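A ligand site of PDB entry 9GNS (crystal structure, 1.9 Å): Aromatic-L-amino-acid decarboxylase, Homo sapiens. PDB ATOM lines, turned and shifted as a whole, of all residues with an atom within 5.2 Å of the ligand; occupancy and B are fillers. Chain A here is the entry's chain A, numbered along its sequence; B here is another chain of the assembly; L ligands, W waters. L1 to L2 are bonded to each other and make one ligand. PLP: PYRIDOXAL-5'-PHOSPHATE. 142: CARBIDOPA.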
ATOM      1  N   TRP A  71     -28.092 -23.154 -24.261  1.00  0.00           N
ATOM      2  CA  TRP A  71     -28.245 -22.847 -22.833  1.00  0.00           C
ATOM      3  C   TRP A  71     -29.379 -23.617 -22.186  1.00  0.00           C
ATOM      4  O   TRP A  71     -29.372 -23.846 -20.965  1.00  0.00           O
ATOM      5  CB  TRP A  71     -28.522 -21.356 -22.638  1.00  0.00           C
ATOM      6  CG  TRP A  71     -27.317 -20.478 -22.711  1.00  0.00           C
ATOM      7  CD1 TRP A  71     -26.595 -20.161 -23.830  1.00  0.00           C
ATOM      8  CD2 TRP A  71     -26.677 -19.817 -21.621  1.00  0.00           C
ATOM      9  NE1 TRP A  71     -25.559 -19.324 -23.497  1.00  0.00           N
ATOM     10  CE2 TRP A  71     -25.578 -19.103 -22.139  1.00  0.00           C
ATOM     11  CE3 TRP A  71     -26.927 -19.761 -20.242  1.00  0.00           C
ATOM     12  CZ2 TRP A  71     -24.733 -18.333 -21.337  1.00  0.00           C
ATOM     13  CZ3 TRP A  71     -26.085 -18.999 -19.443  1.00  0.00           C
ATOM     14  CH2 TRP A  71     -25.002 -18.292 -19.992  1.00  0.00           C
ATOM     15  N   TYR A  79     -21.685 -21.982 -16.288  1.00  0.00           N
ATOM     16  CA  TYR A  79     -21.988 -20.662 -15.739  1.00  0.00           C
ATOM     17  C   TYR A  79     -23.073 -20.729 -14.671  1.00  0.00           C
ATOM     18  O   TYR A  79     -22.904 -21.371 -13.631  1.00  0.00           O
ATOM     19  CB  TYR A  79     -22.385 -19.701 -16.869  1.00  0.00           C
ATOM     20  CG  TYR A  79     -21.501 -19.798 -18.102  1.00  0.00           C
ATOM     21  CD1 TYR A  79     -20.163 -19.404 -18.061  1.00  0.00           C
ATOM     22  CD2 TYR A  79     -22.016 -20.232 -19.324  1.00  0.00           C
ATOM     23  CE1 TYR A  79     -19.353 -19.480 -19.189  1.00  0.00           C
ATOM     24  CE2 TYR A  79     -21.204 -20.316 -20.464  1.00  0.00           C
ATOM     25  CZ  TYR A  79     -19.877 -19.934 -20.375  1.00  0.00           C
ATOM     26  OH  TYR A  79     -19.070 -19.981 -21.487  1.00  0.00           O
ATOM     27  N   PHE A  80     -24.188 -20.049 -14.917  1.00  0.00           N
ATOM     28  CA  PHE A  80     -25.401 -20.106 -14.135  1.00  0.00           C
ATOM     29  C   PHE A  80     -26.554 -20.229 -15.128  1.00  0.00           C
ATOM     30  O   PHE A  80     -26.396 -19.874 -16.296  1.00  0.00           O
ATOM     31  CB  PHE A  80     -25.579 -18.837 -13.276  1.00  0.00           C
ATOM     32  CG  PHE A  80     -24.828 -18.856 -11.967  1.00  0.00           C
ATOM     33  CD1 PHE A  80     -24.736 -20.008 -11.208  1.00  0.00           C
ATOM     34  CD2 PHE A  80     -24.226 -17.702 -11.491  1.00  0.00           C
ATOM     35  CE1 PHE A  80     -24.048 -20.015 -10.001  1.00  0.00           C
ATOM     36  CE2 PHE A  80     -23.531 -17.698 -10.290  1.00  0.00           C
ATOM     37  CZ  PHE A  80     -23.438 -18.857  -9.543  1.00  0.00           C
ATOM     38  N   PRO A  81     -27.708 -20.727 -14.700  1.00  0.00           N
ATOM     39  CA  PRO A  81     -28.850 -20.746 -15.622  1.00  0.00           C
ATOM     40  C   PRO A  81     -29.167 -19.348 -16.139  1.00  0.00           C
ATOM     41  O   PRO A  81     -28.934 -18.344 -15.455  1.00  0.00           O
ATOM     42  CB  PRO A  81     -30.004 -21.295 -14.760  1.00  0.00           C
ATOM     43  CG  PRO A  81     -29.598 -20.982 -13.344  1.00  0.00           C
ATOM     44  CD  PRO A  81     -28.089 -21.152 -13.343  1.00  0.00           C
ATOM     45  N   THR A  82     -29.680 -19.295 -17.360  1.00  0.00           N
ATOM     46  CA  THR A  82     -30.421 -18.124 -17.776  1.00  0.00           C
ATOM     47  C   THR A  82     -31.862 -18.546 -18.023  1.00  0.00           C
ATOM     48  O   THR A  82     -32.140 -19.731 -18.275  1.00  0.00           O
ATOM     49  CB  THR A  82     -29.813 -17.446 -19.026  1.00  0.00           C
ATOM     50  OG1 THR A  82     -30.353 -16.114 -19.144  1.00  0.00           O
ATOM     51  CG2 THR A  82     -30.164 -18.209 -20.289  1.00  0.00           C
ATOM     52  N   ALA A  83     -32.772 -17.596 -17.902  1.00  0.00           N
ATOM     53  CA  ALA A  83     -34.195 -17.905 -17.852  1.00  0.00           C
ATOM     54  C   ALA A  83     -34.760 -18.189 -19.232  1.00  0.00           C
ATOM     55  O   ALA A  83     -34.455 -17.493 -20.210  1.00  0.00           O
ATOM     56  CB  ALA A  83     -34.962 -16.753 -17.206  1.00  0.00           C
ATOM     57  N   GLY A 146     -31.325  -3.516 -16.922  1.00  0.00           N
ATOM     58  CA  GLY A 146     -31.032  -4.446 -18.005  1.00  0.00           C
ATOM     59  C   GLY A 146     -30.181  -5.630 -17.590  1.00  0.00           C
ATOM     60  O   GLY A 146     -30.224  -6.675 -18.244  1.00  0.00           O
ATOM     61  N   SER A 147     -29.432  -5.493 -16.504  1.00  0.00           N
ATOM     62  CA  SER A 147     -28.483  -6.511 -16.089  1.00  0.00           C
ATOM     63  C   SER A 147     -27.987  -6.165 -14.693  1.00  0.00           C
ATOM     64  O   SER A 147     -28.059  -5.012 -14.266  1.00  0.00           O
ATOM     65  CB  SER A 147     -27.328  -6.615 -17.083  1.00  0.00           C
ATOM     66  OG  SER A 147     -26.460  -5.501 -16.966  1.00  0.00           O
ATOM     67  N   ALA A 148     -27.495  -7.186 -13.989  1.00  0.00           N
ATOM     68  CA  ALA A 148     -26.900  -6.942 -12.682  1.00  0.00           C
ATOM     69  C   ALA A 148     -25.621  -6.123 -12.813  1.00  0.00           C
ATOM     70  O   ALA A 148     -25.286  -5.354 -11.900  1.00  0.00           O
ATOM     71  CB  ALA A 148     -26.621  -8.266 -11.955  1.00  0.00           C
ATOM     72  N   SER A 149     -24.891  -6.281 -13.914  1.00  0.00           N
ATOM     73  CA  SER A 149     -23.698  -5.468 -14.139  1.00  0.00           C
ATOM     74  C   SER A 149     -24.065  -4.007 -14.188  1.00  0.00           C
ATOM     75  O   SER A 149     -23.364  -3.157 -13.632  1.00  0.00           O
ATOM     76  CB  SER A 149     -22.997  -5.884 -15.428  1.00  0.00           C
ATOM     77  OG  SER A 149     -22.609  -7.243 -15.405  1.00  0.00           O
ATOM     78  N   GLU A 150     -25.175  -3.690 -14.861  1.00  0.00           N
ATOM     79  CA  GLU A 150     -25.634  -2.315 -14.924  1.00  0.00           C
ATOM     80  C   GLU A 150     -26.147  -1.856 -13.555  1.00  0.00           C
ATOM     81  O   GLU A 150     -25.926  -0.713 -13.159  1.00  0.00           O
ATOM     82  CB  GLU A 150     -26.739  -2.168 -15.973  1.00  0.00           C
ATOM     83  CG  GLU A 150     -26.213  -2.158 -17.395  1.00  0.00           C
ATOM     84  CD  GLU A 150     -27.281  -2.544 -18.416  1.00  0.00           C
ATOM     85  OE1 GLU A 150     -27.903  -1.613 -18.961  1.00  0.00           O
ATOM     86  OE2 GLU A 150     -27.520  -3.750 -18.644  1.00  0.00           O
ATOM     87  N   HIS A 192     -17.939 -10.747  -8.888  1.00  0.00           N
ATOM     88  CA  HIS A 192     -18.044 -10.828 -10.337  1.00  0.00           C
ATOM     89  C   HIS A 192     -17.289  -9.676 -10.983  1.00  0.00           C
ATOM     90  O   HIS A 192     -17.127  -8.600 -10.404  1.00  0.00           O
ATOM     91  CB  HIS A 192     -19.526 -10.802 -10.743  1.00  0.00           C
ATOM     92  CG  HIS A 192     -19.760 -11.032 -12.212  1.00  0.00           C
ATOM     93  ND1 HIS A 192     -20.018 -10.006 -13.091  1.00  0.00           N
ATOM     94  CD2 HIS A 192     -19.775 -12.172 -12.940  1.00  0.00           C
ATOM     95  CE1 HIS A 192     -20.193 -10.498 -14.310  1.00  0.00           C
ATOM     96  NE2 HIS A 192     -20.038 -11.806 -14.244  1.00  0.00           N
ATOM     97  N   SER A 194     -18.188  -7.649 -13.000  1.00  0.00           N
ATOM     98  CA  SER A 194     -18.997  -6.443 -13.138  1.00  0.00           C
ATOM     99  C   SER A 194     -18.635  -5.393 -12.100  1.00  0.00           C
ATOM    100  O   SER A 194     -18.826  -4.192 -12.337  1.00  0.00           O
ATOM    101  CB  SER A 194     -20.486  -6.782 -13.034  1.00  0.00           C
ATOM    102  OG  SER A 194     -20.734  -7.579 -11.885  1.00  0.00           O
ATOM    103  N   THR A 242     -21.618  -9.878  -1.956  1.00  0.00           N
ATOM    104  CA  THR A 242     -22.180 -10.838  -2.896  1.00  0.00           C
ATOM    105  C   THR A 242     -22.849 -11.985  -2.156  1.00  0.00           C
ATOM    106  O   THR A 242     -22.256 -12.586  -1.256  1.00  0.00           O
ATOM    107  CB  THR A 242     -21.103 -11.380  -3.837  1.00  0.00           C
ATOM    108  OG1 THR A 242     -20.440 -10.291  -4.502  1.00  0.00           O
ATOM    109  CG2 THR A 242     -21.704 -12.325  -4.879  1.00  0.00           C
ATOM    110  N   GLY A 244     -24.077 -15.476  -3.260  1.00  0.00           N
ATOM    111  CA  GLY A 244     -24.005 -16.410  -4.374  1.00  0.00           C
ATOM    112  C   GLY A 244     -22.920 -16.067  -5.375  1.00  0.00           C
ATOM    113  O   GLY A 244     -23.216 -15.702  -6.516  1.00  0.00           O
ATOM    114  N   THR A 245     -21.656 -16.189  -4.961  1.00  0.00           N
ATOM    115  CA  THR A 245     -20.554 -15.762  -5.804  1.00  0.00           C
ATOM    116  C   THR A 245     -20.514 -16.593  -7.088  1.00  0.00           C
ATOM    117  O   THR A 245     -20.906 -17.761  -7.120  1.00  0.00           O
ATOM    118  CB  THR A 245     -19.217 -15.887  -5.070  1.00  0.00           C
ATOM    119  OG1 THR A 245     -19.035 -17.227  -4.589  1.00  0.00           O
ATOM    120  CG2 THR A 245     -19.179 -14.913  -3.890  1.00  0.00           C
ATOM    121  N   THR A 246     -20.033 -15.957  -8.158  1.00  0.00           N
ATOM    122  CA  THR A 246     -19.998 -16.612  -9.463  1.00  0.00           C
ATOM    123  C   THR A 246     -19.077 -17.822  -9.455  1.00  0.00           C
ATOM    124  O   THR A 246     -19.337 -18.807 -10.169  1.00  0.00           O
ATOM    125  CB  THR A 246     -19.549 -15.612 -10.528  1.00  0.00           C
ATOM    126  OG1 THR A 246     -20.133 -14.335 -10.255  1.00  0.00           O
ATOM    127  CG2 THR A 246     -19.982 -16.069 -11.919  1.00  0.00           C
ATOM    128  N   ASP A 271     -25.259  -7.718  -4.117  1.00  0.00           N
ATOM    129  CA  ASP A 271     -25.355  -8.377  -5.414  1.00  0.00           C
ATOM    130  C   ASP A 271     -25.700  -9.837  -5.164  1.00  0.00           C
ATOM    131  O   ASP A 271     -24.868 -10.606  -4.682  1.00  0.00           O
ATOM    132  CB  ASP A 271     -24.039  -8.220  -6.164  1.00  0.00           C
ATOM    133  CG  ASP A 271     -23.919  -9.133  -7.386  1.00  0.00           C
ATOM    134  OD1 ASP A 271     -24.906  -9.769  -7.800  1.00  0.00           O
ATOM    135  OD2 ASP A 271     -22.810  -9.178  -7.966  1.00  0.00           O
ATOM    136  N   ALA A 273     -27.112 -11.775  -7.805  1.00  0.00           N
ATOM    137  CA  ALA A 273     -27.559 -12.022  -9.181  1.00  0.00           C
ATOM    138  C   ALA A 273     -28.215 -13.382  -9.368  1.00  0.00           C
ATOM    139  O   ALA A 273     -29.336 -13.481  -9.887  1.00  0.00           O
ATOM    140  CB  ALA A 273     -26.373 -11.874 -10.133  1.00  0.00           C
ATOM    141  N   TYR A 274     -27.527 -14.444  -8.953  1.00  0.00           N
ATOM    142  CA  TYR A 274     -28.027 -15.805  -9.127  1.00  0.00           C
ATOM    143  C   TYR A 274     -28.865 -16.251  -7.941  1.00  0.00           C
ATOM    144  O   TYR A 274     -30.026 -16.644  -8.093  1.00  0.00           O
ATOM    145  CB  TYR A 274     -26.855 -16.778  -9.338  1.00  0.00           C
ATOM    146  CG  TYR A 274     -27.230 -18.228  -9.121  1.00  0.00           C
ATOM    147  CD1 TYR A 274     -28.081 -18.876 -10.012  1.00  0.00           C
ATOM    148  CD2 TYR A 274     -26.761 -18.933  -8.030  1.00  0.00           C
ATOM    149  CE1 TYR A 274     -28.438 -20.210  -9.830  1.00  0.00           C
ATOM    150  CE2 TYR A 274     -27.106 -20.254  -7.829  1.00  0.00           C
ATOM    151  CZ  TYR A 274     -27.947 -20.889  -8.735  1.00  0.00           C
ATOM    152  OH  TYR A 274     -28.289 -22.208  -8.543  1.00  0.00           O
ATOM    153  N   ASN A 300     -31.090 -11.226 -10.343  1.00  0.00           N
ATOM    154  CA  ASN A 300     -31.542 -11.391 -11.727  1.00  0.00           C
ATOM    155  C   ASN A 300     -32.655 -12.419 -11.822  1.00  0.00           C
ATOM    156  O   ASN A 300     -32.375 -13.633 -11.793  1.00  0.00           O
ATOM    157  CB  ASN A 300     -30.367 -11.828 -12.615  1.00  0.00           C
ATOM    158  CG  ASN A 300     -29.418 -10.704 -12.893  1.00  0.00           C
ATOM    159  OD1 ASN A 300     -29.762  -9.536 -12.759  1.00  0.00           O
ATOM    160  ND2 ASN A 300     -28.197 -11.058 -13.267  1.00  0.00           N
ATOM    161  N   HIS A 302     -33.687 -12.952 -14.554  1.00  0.00           N
ATOM    162  CA  HIS A 302     -33.319 -13.577 -15.820  1.00  0.00           C
ATOM    163  C   HIS A 302     -32.227 -14.636 -15.673  1.00  0.00           C
ATOM    164  O   HIS A 302     -31.839 -15.232 -16.691  1.00  0.00           O
ATOM    165  CB  HIS A 302     -32.942 -12.524 -16.872  1.00  0.00           C
ATOM    166  CG  HIS A 302     -31.673 -11.769 -16.621  1.00  0.00           C
ATOM    167  ND1 HIS A 302     -31.557 -10.424 -16.894  1.00  0.00           N
ATOM    168  CD2 HIS A 302     -30.446 -12.162 -16.190  1.00  0.00           C
ATOM    169  CE1 HIS A 302     -30.328 -10.018 -16.621  1.00  0.00           C
ATOM    170  NE2 HIS A 302     -29.639 -11.058 -16.179  1.00  0.00           N
ATOM    171  N   LYS A 303     -31.757 -14.917 -14.461  1.00  0.00           N
ATOM    172  CA  LYS A 303     -30.956 -16.128 -14.239  1.00  0.00           C
ATOM    173  C   LYS A 303     -31.886 -17.254 -13.786  1.00  0.00           C
ATOM    174  O   LYS A 303     -32.134 -18.203 -14.520  1.00  0.00           O
ATOM    175  CB  LYS A 303     -29.842 -15.884 -13.205  1.00  0.00           C
ATOM    176  CG  LYS A 303     -28.616 -15.198 -13.763  1.00  0.00           C
ATOM    177  CD  LYS A 303     -27.522 -15.126 -12.696  1.00  0.00           C
ATOM    178  CE  LYS A 303     -26.226 -14.571 -13.262  1.00  0.00           C
ATOM    179  NZ  LYS A 303     -26.472 -13.310 -14.032  1.00  0.00           N
ATOM    180  N   PHE A 309     -34.080 -13.050 -20.126  1.00  0.00           N
ATOM    181  CA  PHE A 309     -33.240 -11.867 -20.306  1.00  0.00           C
ATOM    182  C   PHE A 309     -33.840 -10.935 -21.353  1.00  0.00           C
ATOM    183  O   PHE A 309     -34.362 -11.382 -22.370  1.00  0.00           O
ATOM    184  CB  PHE A 309     -31.839 -12.350 -20.739  1.00  0.00           C
ATOM    185  CG  PHE A 309     -30.786 -11.276 -20.749  1.00  0.00           C
ATOM    186  CD1 PHE A 309     -30.685 -10.391 -21.822  1.00  0.00           C
ATOM    187  CD2 PHE A 309     -29.863 -11.186 -19.730  1.00  0.00           C
ATOM    188  CE1 PHE A 309     -29.684  -9.418 -21.843  1.00  0.00           C
ATOM    189  CE2 PHE A 309     -28.863 -10.205 -19.739  1.00  0.00           C
ATOM    190  CZ  PHE A 309     -28.782  -9.329 -20.800  1.00  0.00           C
ATOM    191  N   ILE B 101     -26.997 -15.990 -23.750  1.00  0.00           N
ATOM    192  CA  ILE B 101     -26.405 -14.755 -23.240  1.00  0.00           C
ATOM    193  C   ILE B 101     -25.036 -14.631 -23.884  1.00  0.00           C
ATOM    194  O   ILE B 101     -24.103 -15.346 -23.492  1.00  0.00           O
ATOM    195  CB  ILE B 101     -26.307 -14.756 -21.711  1.00  0.00           C
ATOM    196  CG1 ILE B 101     -27.651 -15.154 -21.101  1.00  0.00           C
ATOM    197  CG2 ILE B 101     -25.861 -13.369 -21.211  1.00  0.00           C
ATOM    198  CD1 ILE B 101     -28.817 -14.247 -21.533  1.00  0.00           C
ATOM    199  N   PHE B 103     -22.179 -13.137 -23.768  1.00  0.00           N
ATOM    200  CA  PHE B 103     -21.103 -12.371 -23.143  1.00  0.00           C
ATOM    201  C   PHE B 103     -19.720 -12.839 -23.570  1.00  0.00           C
ATOM    202  O   PHE B 103     -18.726 -12.268 -23.132  1.00  0.00           O
ATOM    203  CB  PHE B 103     -21.204 -12.459 -21.619  1.00  0.00           C
ATOM    204  CG  PHE B 103     -21.218 -13.878 -21.105  1.00  0.00           C
ATOM    205  CD1 PHE B 103     -20.030 -14.586 -20.978  1.00  0.00           C
ATOM    206  CD2 PHE B 103     -22.409 -14.506 -20.809  1.00  0.00           C
ATOM    207  CE1 PHE B 103     -20.040 -15.894 -20.529  1.00  0.00           C
ATOM    208  CE2 PHE B 103     -22.413 -15.804 -20.366  1.00  0.00           C
ATOM    209  CZ  PHE B 103     -21.235 -16.493 -20.217  1.00  0.00           C
ATOM    210  N   LEU B 353     -22.308  -6.670 -19.494  1.00  0.00           N
ATOM    211  CA  LEU B 353     -21.588  -7.869 -19.926  1.00  0.00           C
ATOM    212  C   LEU B 353     -22.490  -8.788 -20.728  1.00  0.00           C
ATOM    213  O   LEU B 353     -22.097  -9.281 -21.789  1.00  0.00           O
ATOM    214  CB  LEU B 353     -21.057  -8.649 -18.712  1.00  0.00           C
ATOM    215  CG  LEU B 353     -19.723  -8.342 -18.036  1.00  0.00           C
ATOM    216  CD1 LEU B 353     -18.592  -8.186 -19.054  1.00  0.00           C
ATOM    217  CD2 LEU B 353     -19.875  -7.122 -17.154  1.00  0.00           C
ATOM    218  N   GLY B 354     -23.690  -9.044 -20.215  1.00  0.00           N
ATOM    219  CA  GLY B 354     -24.636  -9.868 -20.927  1.00  0.00           C
ATOM    220  C   GLY B 354     -25.280  -9.139 -22.079  1.00  0.00           C
ATOM    221  O   GLY B 354     -25.322  -7.913 -22.113  1.00  0.00           O
HETATM  222  N1  PLP L   1     -23.055 -10.748 -10.070  1.00  0.00           N
HETATM  223  C2  PLP L   1     -22.906 -12.103 -10.116  1.00  0.00           C
HETATM  224  C2A PLP L   1     -22.621 -12.860  -8.860  1.00  0.00           C
HETATM  225  C3  PLP L   1     -23.011 -12.766 -11.329  1.00  0.00           C
HETATM  226  O3  PLP L   1     -22.857 -14.127 -11.363  1.00  0.00           O
HETATM  227  C4  PLP L   1     -23.275 -12.048 -12.495  1.00  0.00           C
HETATM  228  C4A PLP L   1     -23.164 -12.692 -13.843  1.00  0.00           C
HETATM  229  C5  PLP L   1     -23.410 -10.672 -12.427  1.00  0.00           C
HETATM  230  C6  PLP L   1     -23.309 -10.018 -11.218  1.00  0.00           C
HETATM  231  C5A PLP L   1     -23.722  -9.903 -13.692  1.00  0.00           C
HETATM  232  O4P PLP L   1     -25.037 -10.237 -14.088  1.00  0.00           O
HETATM  233  P   PLP L   1     -25.534  -9.802 -15.557  1.00  0.00           P
HETATM  234  O1P PLP L   1     -27.032  -9.619 -15.539  1.00  0.00           O
HETATM  235  O2P PLP L   1     -24.834  -8.486 -15.860  1.00  0.00           O
HETATM  236  O3P PLP L   1     -25.143 -10.852 -16.579  1.00  0.00           O
HETATM  237  NN  142 L   2     -22.303 -14.250 -15.130  1.00  0.00           N
HETATM  238  N   142 L   2     -23.188 -14.106 -14.032  1.00  0.00           N
HETATM  239  CA  142 L   2     -22.126 -15.657 -15.563  1.00  0.00           C
HETATM  240  CB  142 L   2     -22.755 -15.652 -16.978  1.00  0.00           C
HETATM  241  CB1 142 L   2     -22.624 -16.724 -14.577  1.00  0.00           C
HETATM  242  CG  142 L   2     -24.281 -15.450 -17.023  1.00  0.00           C
HETATM  243  CD1 142 L   2     -24.789 -14.179 -17.250  1.00  0.00           C
HETATM  244  CE1 142 L   2     -26.174 -13.977 -17.300  1.00  0.00           C
HETATM  245  CD2 142 L   2     -25.153 -16.530 -16.880  1.00  0.00           C
HETATM  246  CE2 142 L   2     -26.539 -16.328 -16.930  1.00  0.00           C
HETATM  247  CZ  142 L   2     -27.045 -15.041 -17.142  1.00  0.00           C
HETATM  248  OH  142 L   2     -28.477 -14.797 -17.204  1.00  0.00           O
HETATM  249  OE1 142 L   2     -26.721 -12.661 -17.524  1.00  0.00           O
HETATM  250  C   142 L   2     -20.626 -15.705 -15.874  1.00  0.00           C
HETATM  251  O   142 L   2     -20.126 -16.722 -16.365  1.00  0.00           O
HETATM  252  OXT 142 L   2     -19.916 -14.724 -15.609  1.00  0.00           O
HETATM  253  O   HOH W   1     -24.459  -7.380 -18.078  1.00  0.00           O
HETATM  254  O   HOH W   2     -22.834 -11.206 -17.611  1.00  0.00           O
HETATM  255  O   HOH W   3     -17.525 -14.806 -14.065  1.00  0.00           O
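The backbone NH (N) of Ser 149 sits at hydrogen-bond distance from an oxygen (O2P) of PLP L1 (2.9 Å). An oxygen (O2P) of PLP L1 sits at hydrogen-bond distance from the side-chain hydroxyl of Ser 149. The side-chain carboxylate (OD2) of Asp 271 sits at hydrogen-bond distance from a nitrogen (N1) of PLP L1 (2.6 Å). The backbone NH (N) of Ala 148 lies within hydrogen-bond range of an oxygen (O1P) of PLP L1, 2.9 Å away. An oxygen (O1P) of PLP L1 is in hydrogen-bond range of the side-chain amide nitrogen (ND2) of Asn 300 (2.9 Å). O3 of PLP L1 sits at hydrogen-bond distance from OG1 of Thr 246. OG1 of Thr 82 lies within hydrogen-bond range of OH of 142 L2, 3.0 Å away. An oxygen (OH) of 142 L2 is in hydrogen-bond range of the backbone carbonyl oxygen (O) of His 302 (3.4 Å). An oxygen (O1P) of PLP L1 sits at hydrogen-bond distance from a ring nitrogen (NE2) of His 302 (3.0 Å). NZ of Lys 303 is in salt-bridge range of O3P of PLP L1 (3.8 Å). A ring nitrogen (NE2) of His 192 lies within hydrogen-bond range of an oxygen (OXT) of 142 L2 (3.2 Å).
Water W1 lies within hydrogen-bond range of O2P of PLP L1 (2.5 Å), N of Leu 353 of chain B (2.7 Å), N of Gly 354 of chain B (2.8 Å), OG of Ser 147 (3.0 Å) and OG of Ser 149 (3.3 Å). Water W2 bridges an oxygen (O3P) of PLP L1 and the backbone NH of Gly 354 of chain B.
Merely in contact with the ligand: Trp 71, Tyr 79, Phe 80, Pro 81, Ser 147, Ser 194, Gly 244, Ala 273, Phe 309, Ile 101 of chain B and Phe 103 of chain B. Hydrophobic or aromatic side chains that line the ligand: Trp 71, Tyr 79, Phe 80, Ala 148, His 192, Ala 273, His 302, Phe 309, Ile 101 of chain B and Phe 103 of chain B. Within 4 Å of the ligand: Trp 71, Tyr 79, Phe 80, Pro 81, Thr 82, Ser 147, Ala 148, Ser 149, His 192, Ser 194, Gly 244, Thr 246, Asp 271, Ala 273, Asn 300, His 302, Lys 303, Phe 309, Ile 101 of chain B and Phe 103 of chain B. The nearest printed residue that does not touch the ligand is Thr 242 (4.1 Å).
N of Ala 148 sits close to OD1 of Asn 300, 3.5 Å away. ND2 of Asn 300 lies within hydrogen-bond range of NE2 of His 302, 3.2 Å away. NZ of Lys 303 lies close to ND2 of Asn 300, at 2.9 Å. The backbone NH of Asn 300 sits at hydrogen-bond distance from the backbone carbonyl oxygen of Ala 273, 2.9 Å away. The side-chain hydroxyl of Thr 82 sits at hydrogen-bond distance from the backbone carbonyl oxygen of His 302 (3.0 Å). O of Lys 303 lies within hydrogen-bond range of N of Ala 83. The side-chain hydroxyl of Ser 194 is in hydrogen-bond range of a ring nitrogen (ND1) of His 192 (2.8 Å). The side-chain carboxylate (OE2) of Glu 150 sits at hydrogen-bond distance from the side-chain hydroxyl (OG) of Ser 147, at 2.6 Å.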
